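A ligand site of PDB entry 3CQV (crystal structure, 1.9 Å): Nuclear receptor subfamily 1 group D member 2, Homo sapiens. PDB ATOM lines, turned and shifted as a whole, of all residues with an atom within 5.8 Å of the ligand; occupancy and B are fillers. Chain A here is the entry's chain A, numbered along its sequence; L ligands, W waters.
The side-chain sulfur of Cys 4 lies close to the backbone NH of Met 6, at 3.5 Å.
Water W3 lies within hydrogen-bond range of an oxygen (O3) of the ligand (2.5 Å), the side-chain carboxylate (OE1) of Glu 191 (3.2 Å) and the backbone carbonyl oxygen (O) of Gly 98 (3.3 Å).
Water W1 bridges O3 of the ligand (2.6 Å) and OE1 of Glu 191 (2.8 Å).
Water W4 bridges an oxygen (O1) of the ligand and the backbone carbonyl oxygen (O) of Met 97.
Water W5 lies within hydrogen-bond range of the backbone carbonyl oxygen (O) of Glu 191 (2.8 Å), an oxygen (O2) of the ligand (2.9 Å) and the backbone NH (N) of Phe 195 (3.5 Å).
Water W2 bridges the backbone carbonyl oxygen of Gly 98 (2.9 Å) and an oxygen (O2) of the ligand (3.1 Å).
An iron atom (FE1) of the ligand is bound by a ring nitrogen (NE2) of His 188 (2.2 Å).
The side-chain sulfur of Cys 4 binds an iron atom (FE1) of the ligand (2.3 Å).
N of Gly 100 sits at hydrogen-bond distance from O4 of the ligand, at 2.8 Å.
The backbone NH (N) of Leu 103 is in hydrogen-bond range of an oxygen (O4) of the ligand.
N of Val 3 is in hydrogen-bond range of O1 of the ligand (2.8 Å).
An oxygen (O1) of the ligand lies close to the backbone carbonyl oxygen of His 1, at 3.2 Å.
Merely in contact with the ligand: Phe 29 (3.3 Å), Leu 2 (3.3 Å), Met 106 (3.3 Å), Phe 25 (3.3 Å), Met 6 (3.3 Å), Leu 66 (3.4 Å), Pro 5 (3.4 Å), Ala 99 (3.5 Å), Val 33 (3.6 Å), Leu 102 (3.6 Å), Phe 63 (3.6 Å), Met 67 (3.6 Å), Phe 195 (3.7 Å), Phe 74 (3.7 Å), Glu 191 (3.7 Å), Phe 70 (3.8 Å), Trp 22 (3.8 Å), Leu 192 (3.8 Å) and Gly 98 (3.9 Å).
Hydrophobic or aromatic side chains that line the ligand: Leu 2, Val 3, Pro 5, Met 6, Trp 22, Phe 25, Phe 29, Val 33, Phe 63, Leu 66, Met 67, Phe 70, Phe 74, Ala 99, Leu 102, Leu 103, Met 106, His 188, Leu 192 and Phe 195.
Of the 32 residues printed, 25 come within 4 Å of the ligand.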
ATOM      1  N   HIS A   1      34.917  24.125  25.709  1.00  0.00           N
ATOM      2  CA  HIS A   1      34.298  23.557  24.464  1.00  0.00           C
ATOM      3  C   HIS A   1      32.805  23.206  24.580  1.00  0.00           C
ATOM      4  O   HIS A   1      32.294  22.847  25.649  1.00  0.00           O
ATOM      5  CB  HIS A   1      35.098  22.344  23.961  1.00  0.00           C
ATOM      6  CG  HIS A   1      36.560  22.612  23.813  1.00  0.00           C
ATOM      7  ND1 HIS A   1      37.497  22.173  24.722  1.00  0.00           N
ATOM      8  CD2 HIS A   1      37.248  23.305  22.865  1.00  0.00           C
ATOM      9  CE1 HIS A   1      38.696  22.559  24.327  1.00  0.00           C
ATOM     10  NE2 HIS A   1      38.573  23.255  23.224  1.00  0.00           N
ATOM     11  N   LEU A   2      32.140  23.308  23.435  1.00  0.00           N
ATOM     12  CA  LEU A   2      30.734  22.939  23.286  1.00  0.00           C
ATOM     13  C   LEU A   2      30.692  22.014  22.051  1.00  0.00           C
ATOM     14  O   LEU A   2      30.633  22.469  20.909  1.00  0.00           O
ATOM     15  CB  LEU A   2      29.889  24.226  23.153  1.00  0.00           C
ATOM     16  CG  LEU A   2      28.435  24.336  22.662  1.00  0.00           C
ATOM     17  CD1 LEU A   2      27.673  23.026  22.673  1.00  0.00           C
ATOM     18  CD2 LEU A   2      27.697  25.417  23.413  1.00  0.00           C
ATOM     19  N   VAL A   3      30.723  20.702  22.308  1.00  0.00           N
ATOM     20  CA  VAL A   3      30.987  19.744  21.249  1.00  0.00           C
ATOM     21  C   VAL A   3      29.715  19.226  20.563  1.00  0.00           C
ATOM     22  O   VAL A   3      29.664  18.096  20.062  1.00  0.00           O
ATOM     23  CB  VAL A   3      31.892  18.575  21.709  1.00  0.00           C
ATOM     24  CG1 VAL A   3      33.308  19.094  22.044  1.00  0.00           C
ATOM     25  CG2 VAL A   3      31.299  17.793  22.910  1.00  0.00           C
ATOM     26  N   CYS A   4      28.696  20.065  20.537  1.00  0.00           N
ATOM     27  CA  CYS A   4      27.437  19.697  19.858  1.00  0.00           C
ATOM     28  C   CYS A   4      27.434  20.338  18.485  1.00  0.00           C
ATOM     29  O   CYS A   4      27.628  21.569  18.390  1.00  0.00           O
ATOM     30  CB  CYS A   4      26.276  20.219  20.678  1.00  0.00           C
ATOM     31  SG  CYS A   4      24.677  20.006  19.919  1.00  0.00           S
ATOM     32  N   PRO A   5      27.242  19.536  17.410  1.00  0.00           N
ATOM     33  CA  PRO A   5      27.223  20.068  16.055  1.00  0.00           C
ATOM     34  C   PRO A   5      26.063  21.001  15.716  1.00  0.00           C
ATOM     35  O   PRO A   5      26.039  21.542  14.642  1.00  0.00           O
ATOM     36  CB  PRO A   5      27.196  18.812  15.170  1.00  0.00           C
ATOM     37  CG  PRO A   5      26.524  17.785  16.036  1.00  0.00           C
ATOM     38  CD  PRO A   5      27.095  18.056  17.400  1.00  0.00           C
ATOM     39  N   MET A   6      25.127  21.214  16.631  1.00  0.00           N
ATOM     40  CA  MET A   6      24.127  22.259  16.406  1.00  0.00           C
ATOM     41  C   MET A   6      24.773  23.633  16.590  1.00  0.00           C
ATOM     42  O   MET A   6      24.152  24.629  16.241  1.00  0.00           O
ATOM     43  CB  MET A   6      22.939  22.122  17.346  1.00  0.00           C
ATOM     44  CG  MET A   6      22.200  20.806  17.255  1.00  0.00           C
ATOM     45  SD  MET A   6      21.356  20.604  15.536  1.00  0.00           S
ATOM     46  CE  MET A   6      22.655  19.363  14.733  1.00  0.00           C
ATOM     47  N   TRP A  22      25.053  30.622  25.844  1.00  0.00           N
ATOM     48  CA  TRP A  22      23.758  30.040  25.460  1.00  0.00           C
ATOM     49  C   TRP A  22      22.999  30.809  24.379  1.00  0.00           C
ATOM     50  O   TRP A  22      22.399  30.213  23.466  1.00  0.00           O
ATOM     51  CB  TRP A  22      22.873  29.778  26.670  1.00  0.00           C
ATOM     52  CG  TRP A  22      21.838  28.761  26.316  1.00  0.00           C
ATOM     53  CD1 TRP A  22      20.543  28.979  25.969  1.00  0.00           C
ATOM     54  CD2 TRP A  22      22.054  27.350  26.215  1.00  0.00           C
ATOM     55  NE1 TRP A  22      19.913  27.777  25.681  1.00  0.00           N
ATOM     56  CE2 TRP A  22      20.831  26.765  25.820  1.00  0.00           C
ATOM     57  CE3 TRP A  22      23.166  26.526  26.434  1.00  0.00           C
ATOM     58  CZ2 TRP A  22      20.691  25.387  25.638  1.00  0.00           C
ATOM     59  CZ3 TRP A  22      23.009  25.144  26.266  1.00  0.00           C
ATOM     60  CH2 TRP A  22      21.783  24.596  25.873  1.00  0.00           C
ATOM     61  N   PHE A  25      24.669  30.171  21.115  1.00  0.00           N
ATOM     62  CA  PHE A  25      24.338  28.774  20.744  1.00  0.00           C
ATOM     63  C   PHE A  25      22.890  28.709  20.226  1.00  0.00           C
ATOM     64  O   PHE A  25      22.621  28.132  19.168  1.00  0.00           O
ATOM     65  CB  PHE A  25      24.544  27.885  21.965  1.00  0.00           C
ATOM     66  CG  PHE A  25      24.334  26.409  21.717  1.00  0.00           C
ATOM     67  CD1 PHE A  25      24.675  25.823  20.485  1.00  0.00           C
ATOM     68  CD2 PHE A  25      23.837  25.595  22.738  1.00  0.00           C
ATOM     69  CE1 PHE A  25      24.486  24.449  20.261  1.00  0.00           C
ATOM     70  CE2 PHE A  25      23.640  24.207  22.529  1.00  0.00           C
ATOM     71  CZ  PHE A  25      23.961  23.642  21.293  1.00  0.00           C
ATOM     72  N   PHE A  29      21.035  26.817  16.945  1.00  0.00           N
ATOM     73  CA  PHE A  29      20.106  25.667  16.976  1.00  0.00           C
ATOM     74  C   PHE A  29      18.610  26.029  16.788  1.00  0.00           C
ATOM     75  O   PHE A  29      17.811  25.172  16.363  1.00  0.00           O
ATOM     76  CB  PHE A  29      20.329  24.791  18.232  1.00  0.00           C
ATOM     77  CG  PHE A  29      19.875  25.411  19.543  1.00  0.00           C
ATOM     78  CD1 PHE A  29      18.513  25.632  19.813  1.00  0.00           C
ATOM     79  CD2 PHE A  29      20.786  25.673  20.560  1.00  0.00           C
ATOM     80  CE1 PHE A  29      18.085  26.171  21.019  1.00  0.00           C
ATOM     81  CE2 PHE A  29      20.367  26.227  21.805  1.00  0.00           C
ATOM     82  CZ  PHE A  29      19.021  26.472  22.021  1.00  0.00           C
ATOM     83  N   THR A  30      18.224  27.273  17.103  1.00  0.00           N
ATOM     84  CA  THR A  30      16.814  27.695  17.014  1.00  0.00           C
ATOM     85  C   THR A  30      16.164  27.559  15.625  1.00  0.00           C
ATOM     86  O   THR A  30      15.027  27.094  15.541  1.00  0.00           O
ATOM     87  CB  THR A  30      16.576  29.102  17.629  1.00  0.00           C
ATOM     88  OG1 THR A  30      16.814  29.021  19.039  1.00  0.00           O
ATOM     89  CG2 THR A  30      15.137  29.546  17.432  1.00  0.00           C
ATOM     90  N   VAL A  33      15.129  24.038  15.219  1.00  0.00           N
ATOM     91  CA  VAL A  33      14.011  23.713  16.106  1.00  0.00           C
ATOM     92  C   VAL A  33      12.708  24.205  15.487  1.00  0.00           C
ATOM     93  O   VAL A  33      11.713  23.485  15.478  1.00  0.00           O
ATOM     94  CB  VAL A  33      14.206  24.260  17.537  1.00  0.00           C
ATOM     95  CG1 VAL A  33      12.932  24.064  18.379  1.00  0.00           C
ATOM     96  CG2 VAL A  33      15.370  23.540  18.208  1.00  0.00           C
ATOM     97  N   THR A  62      11.560  16.590  19.454  1.00  0.00           N
ATOM     98  CA  THR A  62      12.336  17.470  18.594  1.00  0.00           C
ATOM     99  C   THR A  62      13.782  16.972  18.462  1.00  0.00           C
ATOM    100  O   THR A  62      14.348  16.948  17.378  1.00  0.00           O
ATOM    101  CB  THR A  62      12.318  18.924  19.134  1.00  0.00           C
ATOM    102  OG1 THR A  62      11.025  19.488  18.850  1.00  0.00           O
ATOM    103  CG2 THR A  62      13.401  19.763  18.454  1.00  0.00           C
ATOM    104  N   PHE A  63      14.386  16.543  19.576  1.00  0.00           N
ATOM    105  CA  PHE A  63      15.748  16.037  19.457  1.00  0.00           C
ATOM    106  C   PHE A  63      15.834  14.838  18.521  1.00  0.00           C
ATOM    107  O   PHE A  63      16.754  14.752  17.741  1.00  0.00           O
ATOM    108  CB  PHE A  63      16.333  15.617  20.818  1.00  0.00           C
ATOM    109  CG  PHE A  63      17.642  14.878  20.664  1.00  0.00           C
ATOM    110  CD1 PHE A  63      18.845  15.578  20.516  1.00  0.00           C
ATOM    111  CD2 PHE A  63      17.656  13.472  20.605  1.00  0.00           C
ATOM    112  CE1 PHE A  63      20.060  14.904  20.342  1.00  0.00           C
ATOM    113  CE2 PHE A  63      18.877  12.783  20.425  1.00  0.00           C
ATOM    114  CZ  PHE A  63      20.070  13.497  20.300  1.00  0.00           C
ATOM    115  N   LEU A  66      15.538  15.887  14.833  1.00  0.00           N
ATOM    116  CA  LEU A  66      16.770  16.478  14.382  1.00  0.00           C
ATOM    117  C   LEU A  66      17.896  15.429  14.268  1.00  0.00           C
ATOM    118  O   LEU A  66      18.744  15.545  13.399  1.00  0.00           O
ATOM    119  CB  LEU A  66      17.182  17.571  15.383  1.00  0.00           C
ATOM    120  CG  LEU A  66      16.264  18.806  15.342  1.00  0.00           C
ATOM    121  CD1 LEU A  66      16.696  19.798  16.390  1.00  0.00           C
ATOM    122  CD2 LEU A  66      16.275  19.446  13.948  1.00  0.00           C
ATOM    123  N   MET A  67      17.937  14.451  15.158  1.00  0.00           N
ATOM    124  CA  MET A  67      18.978  13.406  15.076  1.00  0.00           C
ATOM    125  C   MET A  67      18.884  12.673  13.720  1.00  0.00           C
ATOM    126  O   MET A  67      19.917  12.339  13.082  1.00  0.00           O
ATOM    127  CB  MET A  67      18.857  12.460  16.278  1.00  0.00           C
ATOM    128  CG  MET A  67      19.841  11.300  16.336  1.00  0.00           C
ATOM    129  SD  MET A  67      21.649  12.002  16.725  1.00  0.00           S
ATOM    130  CE  MET A  67      22.461  11.616  15.032  1.00  0.00           C
ATOM    131  N   PHE A  70      19.705  15.234  10.840  1.00  0.00           N
ATOM    132  CA  PHE A  70      21.130  15.585  10.802  1.00  0.00           C
ATOM    133  C   PHE A  70      22.111  14.417  10.935  1.00  0.00           C
ATOM    134  O   PHE A  70      23.308  14.629  11.193  1.00  0.00           O
ATOM    135  CB  PHE A  70      21.440  16.677  11.848  1.00  0.00           C
ATOM    136  CG  PHE A  70      20.896  18.029  11.500  1.00  0.00           C
ATOM    137  CD1 PHE A  70      21.278  18.666  10.318  1.00  0.00           C
ATOM    138  CD2 PHE A  70      20.044  18.696  12.380  1.00  0.00           C
ATOM    139  CE1 PHE A  70      20.800  19.959  10.002  1.00  0.00           C
ATOM    140  CE2 PHE A  70      19.566  19.993  12.088  1.00  0.00           C
ATOM    141  CZ  PHE A  70      19.941  20.612  10.897  1.00  0.00           C
ATOM    142  N   ALA A  71      21.608  13.196  10.751  1.00  0.00           N
ATOM    143  CA  ALA A  71      22.473  12.019  10.740  1.00  0.00           C
ATOM    144  C   ALA A  71      23.552  12.174   9.659  1.00  0.00           C
ATOM    145  O   ALA A  71      24.672  11.676   9.805  1.00  0.00           O
ATOM    146  CB  ALA A  71      21.641  10.754  10.503  1.00  0.00           C
ATOM    147  N   LEU A  73      25.323  14.650   9.047  1.00  0.00           N
ATOM    148  CA  LEU A  73      26.461  15.454   9.523  1.00  0.00           C
ATOM    149  C   LEU A  73      27.621  14.581  10.021  1.00  0.00           C
ATOM    150  O   LEU A  73      28.748  15.060  10.181  1.00  0.00           O
ATOM    151  CB  LEU A  73      26.041  16.390  10.672  1.00  0.00           C
ATOM    152  CG  LEU A  73      24.976  17.474  10.456  1.00  0.00           C
ATOM    153  CD1 LEU A  73      24.818  18.298  11.740  1.00  0.00           C
ATOM    154  CD2 LEU A  73      25.315  18.373   9.273  1.00  0.00           C
ATOM    155  N   PHE A  74      27.336  13.311  10.263  1.00  0.00           N
ATOM    156  CA  PHE A  74      28.280  12.376  10.832  1.00  0.00           C
ATOM    157  C   PHE A  74      28.775  11.543   9.649  1.00  0.00           C
ATOM    158  O   PHE A  74      27.984  10.846   8.997  1.00  0.00           O
ATOM    159  CB  PHE A  74      27.557  11.523  11.887  1.00  0.00           C
ATOM    160  CG  PHE A  74      27.088  12.311  13.073  1.00  0.00           C
ATOM    161  CD1 PHE A  74      27.882  12.427  14.206  1.00  0.00           C
ATOM    162  CD2 PHE A  74      25.844  12.943  13.064  1.00  0.00           C
ATOM    163  CE1 PHE A  74      27.452  13.158  15.303  1.00  0.00           C
ATOM    164  CE2 PHE A  74      25.417  13.688  14.164  1.00  0.00           C
ATOM    165  CZ  PHE A  74      26.235  13.792  15.278  1.00  0.00           C
ATOM    166  N   MET A  97      38.279  17.437  22.987  1.00  0.00           N
ATOM    167  CA  MET A  97      37.455  18.525  23.470  1.00  0.00           C
ATOM    168  C   MET A  97      36.345  18.071  24.417  1.00  0.00           C
ATOM    169  O   MET A  97      35.493  18.883  24.816  1.00  0.00           O
ATOM    170  CB  MET A  97      36.879  19.301  22.295  1.00  0.00           C
ATOM    171  CG  MET A  97      37.907  20.009  21.497  1.00  0.00           C
ATOM    172  SD  MET A  97      37.103  21.152  20.188  1.00  0.00           S
ATOM    173  CE  MET A  97      37.533  20.200  18.532  1.00  0.00           C
ATOM    174  N   GLY A  98      36.347  16.798  24.770  1.00  0.00           N
ATOM    175  CA  GLY A  98      35.398  16.267  25.749  1.00  0.00           C
ATOM    176  C   GLY A  98      34.215  15.465  25.243  1.00  0.00           C
ATOM    177  O   GLY A  98      33.292  15.170  25.998  1.00  0.00           O
ATOM    178  N   ALA A  99      34.191  15.125  23.960  1.00  0.00           N
ATOM    179  CA  ALA A  99      33.134  14.232  23.488  1.00  0.00           C
ATOM    180  C   ALA A  99      33.516  12.823  23.927  1.00  0.00           C
ATOM    181  O   ALA A  99      34.683  12.568  24.250  1.00  0.00           O
ATOM    182  CB  ALA A  99      32.967  14.334  21.996  1.00  0.00           C
ATOM    183  N   GLY A 100      32.550  11.913  23.957  1.00  0.00           N
ATOM    184  CA  GLY A 100      32.807  10.565  24.463  1.00  0.00           C
ATOM    185  C   GLY A 100      31.870   9.558  23.884  1.00  0.00           C
ATOM    186  O   GLY A 100      31.683   9.527  22.661  1.00  0.00           O
ATOM    187  N   ASP A 101      31.289   8.723  24.738  1.00  0.00           N
ATOM    188  CA  ASP A 101      30.480   7.597  24.240  1.00  0.00           C
ATOM    189  C   ASP A 101      29.303   8.074  23.426  1.00  0.00           C
ATOM    190  O   ASP A 101      28.911   7.383  22.478  1.00  0.00           O
ATOM    191  CB  ASP A 101      29.990   6.660  25.345  1.00  0.00           C
ATOM    192  CG  ASP A 101      29.056   5.528  24.813  1.00  0.00           C
ATOM    193  OD1 ASP A 101      29.292   4.955  23.698  1.00  0.00           O
ATOM    194  OD2 ASP A 101      28.072   5.197  25.520  1.00  0.00           O
ATOM    195  N   LEU A 102      28.680   9.187  23.820  1.00  0.00           N
ATOM    196  CA  LEU A 102      27.506   9.627  23.058  1.00  0.00           C
ATOM    197  C   LEU A 102      27.829   9.919  21.588  1.00  0.00           C
ATOM    198  O   LEU A 102      27.143   9.419  20.682  1.00  0.00           O
ATOM    199  CB  LEU A 102      26.810  10.819  23.719  1.00  0.00           C
ATOM    200  CG  LEU A 102      25.595  11.354  22.939  1.00  0.00           C
ATOM    201  CD1 LEU A 102      24.574  10.251  22.584  1.00  0.00           C
ATOM    202  CD2 LEU A 102      24.944  12.466  23.727  1.00  0.00           C
ATOM    203  N   LEU A 103      28.902  10.695  21.351  1.00  0.00           N
ATOM    204  CA  LEU A 103      29.348  10.947  19.988  1.00  0.00           C
ATOM    205  C   LEU A 103      29.572   9.620  19.242  1.00  0.00           C
ATOM    206  O   LEU A 103      29.102   9.468  18.116  1.00  0.00           O
ATOM    207  CB  LEU A 103      30.587  11.854  19.929  1.00  0.00           C
ATOM    208  CG  LEU A 103      31.227  12.100  18.558  1.00  0.00           C
ATOM    209  CD1 LEU A 103      30.265  12.806  17.635  1.00  0.00           C
ATOM    210  CD2 LEU A 103      32.526  12.900  18.675  1.00  0.00           C
ATOM    211  N   ASN A 104      30.232   8.655  19.884  1.00  0.00           N
ATOM    212  CA  ASN A 104      30.441   7.362  19.244  1.00  0.00           C
ATOM    213  C   ASN A 104      29.129   6.688  18.868  1.00  0.00           C
ATOM    214  O   ASN A 104      29.013   6.166  17.752  1.00  0.00           O
ATOM    215  CB  ASN A 104      31.294   6.452  20.143  1.00  0.00           C
ATOM    216  CG  ASN A 104      32.685   7.066  20.423  1.00  0.00           C
ATOM    217  OD1 ASN A 104      33.108   7.997  19.725  1.00  0.00           O
ATOM    218  ND2 ASN A 104      33.366   6.567  21.464  1.00  0.00           N
ATOM    219  N   MET A 106      26.223   8.114  18.307  1.00  0.00           N
ATOM    220  CA  MET A 106      25.634   8.824  17.159  1.00  0.00           C
ATOM    221  C   MET A 106      26.270   8.451  15.839  1.00  0.00           C
ATOM    222  O   MET A 106      25.579   8.396  14.821  1.00  0.00           O
ATOM    223  CB  MET A 106      25.699  10.327  17.388  1.00  0.00           C
ATOM    224  CG  MET A 106      24.838  10.702  18.536  1.00  0.00           C
ATOM    225  SD  MET A 106      24.949  12.612  18.718  1.00  0.00           S
ATOM    226  CE  MET A 106      23.597  12.823  20.096  1.00  0.00           C
ATOM    227  N   HIS A 188      21.820  12.199  25.577  1.00  0.00           N
ATOM    228  CA  HIS A 188      22.041  13.570  25.151  1.00  0.00           C
ATOM    229  C   HIS A 188      21.472  14.581  26.139  1.00  0.00           C
ATOM    230  O   HIS A 188      22.123  15.595  26.415  1.00  0.00           O
ATOM    231  CB  HIS A 188      21.431  13.790  23.783  1.00  0.00           C
ATOM    232  CG  HIS A 188      21.638  15.169  23.264  1.00  0.00           C
ATOM    233  ND1 HIS A 188      20.712  16.171  23.434  1.00  0.00           N
ATOM    234  CD2 HIS A 188      22.676  15.719  22.573  1.00  0.00           C
ATOM    235  CE1 HIS A 188      21.151  17.279  22.870  1.00  0.00           C
ATOM    236  NE2 HIS A 188      22.340  17.035  22.350  1.00  0.00           N
ATOM    237  N   GLU A 191      23.860  15.026  28.898  1.00  0.00           N
ATOM    238  CA  GLU A 191      24.953  15.915  28.487  1.00  0.00           C
ATOM    239  C   GLU A 191      24.501  17.363  28.397  1.00  0.00           C
ATOM    240  O   GLU A 191      25.257  18.261  28.778  1.00  0.00           O
ATOM    241  CB  GLU A 191      25.569  15.507  27.136  1.00  0.00           C
ATOM    242  CG  GLU A 191      26.166  14.091  27.081  1.00  0.00           C
ATOM    243  CD  GLU A 191      27.382  13.923  27.991  1.00  0.00           C
ATOM    244  OE1 GLU A 191      28.235  14.843  28.057  1.00  0.00           O
ATOM    245  OE2 GLU A 191      27.473  12.864  28.668  1.00  0.00           O
ATOM    246  N   LEU A 192      23.300  17.587  27.872  1.00  0.00           N
ATOM    247  CA  LEU A 192      22.787  18.943  27.706  1.00  0.00           C
ATOM    248  C   LEU A 192      22.661  19.617  29.066  1.00  0.00           C
ATOM    249  O   LEU A 192      23.042  20.786  29.220  1.00  0.00           O
ATOM    250  CB  LEU A 192      21.429  18.955  26.988  1.00  0.00           C
ATOM    251  CG  LEU A 192      20.894  20.304  26.475  1.00  0.00           C
ATOM    252  CD1 LEU A 192      19.816  20.059  25.445  1.00  0.00           C
ATOM    253  CD2 LEU A 192      20.349  21.149  27.609  1.00  0.00           C
ATOM    254  N   PHE A 195      25.893  20.749  31.103  1.00  0.00           N
ATOM    255  CA  PHE A 195      26.742  21.753  30.437  1.00  0.00           C
ATOM    256  C   PHE A 195      27.025  22.977  31.323  1.00  0.00           C
ATOM    257  O   PHE A 195      26.116  23.777  31.586  1.00  0.00           O
ATOM    258  CB  PHE A 195      26.120  22.185  29.115  1.00  0.00           C
ATOM    259  CG  PHE A 195      26.957  23.147  28.336  1.00  0.00           C
ATOM    260  CD1 PHE A 195      26.467  24.421  28.027  1.00  0.00           C
ATOM    261  CD2 PHE A 195      28.228  22.802  27.909  1.00  0.00           C
ATOM    262  CE1 PHE A 195      27.228  25.318  27.285  1.00  0.00           C
ATOM    263  CE2 PHE A 195      29.011  23.701  27.166  1.00  0.00           C
ATOM    264  CZ  PHE A 195      28.509  24.954  26.865  1.00  0.00           C
HETATM  265  C1  LIG L   1      26.171  17.538  23.351  1.00  0.00           C
HETATM  266  C2  LIG L   1      22.816  21.042  23.236  1.00  0.00           C
HETATM  267  C3  LIG L   1      20.628  18.879  19.497  1.00  0.00           C
HETATM  268  C4  LIG L   1      24.673  16.255  18.922  1.00  0.00           C
HETATM  269  C5  LIG L   1      25.461  18.671  23.658  1.00  0.00           C
HETATM  270  C6  LIG L   1      25.737  19.574  24.750  1.00  0.00           C
HETATM  271  C7  LIG L   1      24.812  20.571  24.733  1.00  0.00           C
HETATM  272  C8  LIG L   1      23.901  20.292  23.620  1.00  0.00           C
HETATM  273  C9  LIG L   1      24.728  21.796  25.690  1.00  0.00           C
HETATM  274  C10 LIG L   1      26.941  19.378  25.672  1.00  0.00           C
HETATM  275  C11 LIG L   1      28.127  20.058  24.980  1.00  0.00           C
HETATM  276  C12 LIG L   1      29.439  19.922  25.732  1.00  0.00           C
HETATM  277  O1  LIG L   1      30.497  20.208  25.096  1.00  0.00           O
HETATM  278  O2  LIG L   1      29.420  19.497  26.909  1.00  0.00           O
HETATM  279  C13 LIG L   1      21.915  20.762  22.226  1.00  0.00           C
HETATM  280  C14 LIG L   1      20.688  21.481  21.916  1.00  0.00           C
HETATM  281  C15 LIG L   1      20.090  20.864  20.883  1.00  0.00           C
HETATM  282  C16 LIG L   1      20.920  19.744  20.513  1.00  0.00           C
HETATM  283  C17 LIG L   1      20.163  22.734  22.668  1.00  0.00           C
HETATM  284  C18 LIG L   1      18.782  21.156  20.112  1.00  0.00           C
HETATM  285  C19 LIG L   1      18.236  22.383  20.043  1.00  0.00           C
HETATM  286  C20 LIG L   1      21.544  17.974  19.008  1.00  0.00           C
HETATM  287  C21 LIG L   1      21.378  17.161  17.844  1.00  0.00           C
HETATM  288  C22 LIG L   1      22.493  16.446  17.688  1.00  0.00           C
HETATM  289  C23 LIG L   1      23.400  16.782  18.762  1.00  0.00           C
HETATM  290  C24 LIG L   1      20.117  17.132  16.952  1.00  0.00           C
HETATM  291  C25 LIG L   1      22.838  15.420  16.591  1.00  0.00           C
HETATM  292  C26 LIG L   1      22.503  15.629  15.307  1.00  0.00           C
HETATM  293  C27 LIG L   1      25.465  16.344  20.035  1.00  0.00           C
HETATM  294  C28 LIG L   1      26.734  15.661  20.215  1.00  0.00           C
HETATM  295  C29 LIG L   1      27.213  16.035  21.596  1.00  0.00           C
HETATM  296  C30 LIG L   1      26.181  16.933  22.103  1.00  0.00           C
HETATM  297  C31 LIG L   1      27.453  14.746  19.194  1.00  0.00           C
HETATM  298  C32 LIG L   1      28.513  15.584  22.295  1.00  0.00           C
HETATM  299  C33 LIG L   1      28.262  14.127  22.720  1.00  0.00           C
HETATM  300  C34 LIG L   1      29.414  13.589  23.536  1.00  0.00           C
HETATM  301  O3  LIG L   1      29.768  14.246  24.543  1.00  0.00           O
HETATM  302  O4  LIG L   1      29.947  12.500  23.203  1.00  0.00           O
HETATM  303  N1  LIG L   1      24.333  19.105  23.009  1.00  0.00           N
HETATM  304  N2  LIG L   1      22.016  19.693  21.338  1.00  0.00           N
HETATM  305  N3  LIG L   1      22.808  17.741  19.531  1.00  0.00           N
HETATM  306  N4  LIG L   1      25.179  17.061  21.169  1.00  0.00           N
HETATM  307 FE1  LIG L   1      23.587  18.406  21.226  1.00  0.00          FE
HETATM  308  O   HOH W   1      29.250  16.429  25.952  1.00  0.00           O
HETATM  309  O   HOH W   2      31.490  17.162  27.062  1.00  0.00           O
HETATM  310  O   HOH W   3      30.678  13.284  26.609  1.00  0.00           O
HETATM  311  O   HOH W   4      32.918  19.383  26.176  1.00  0.00           O
HETATM  312  O   HOH W   5      27.954  18.633  29.226  1.00  0.00           O
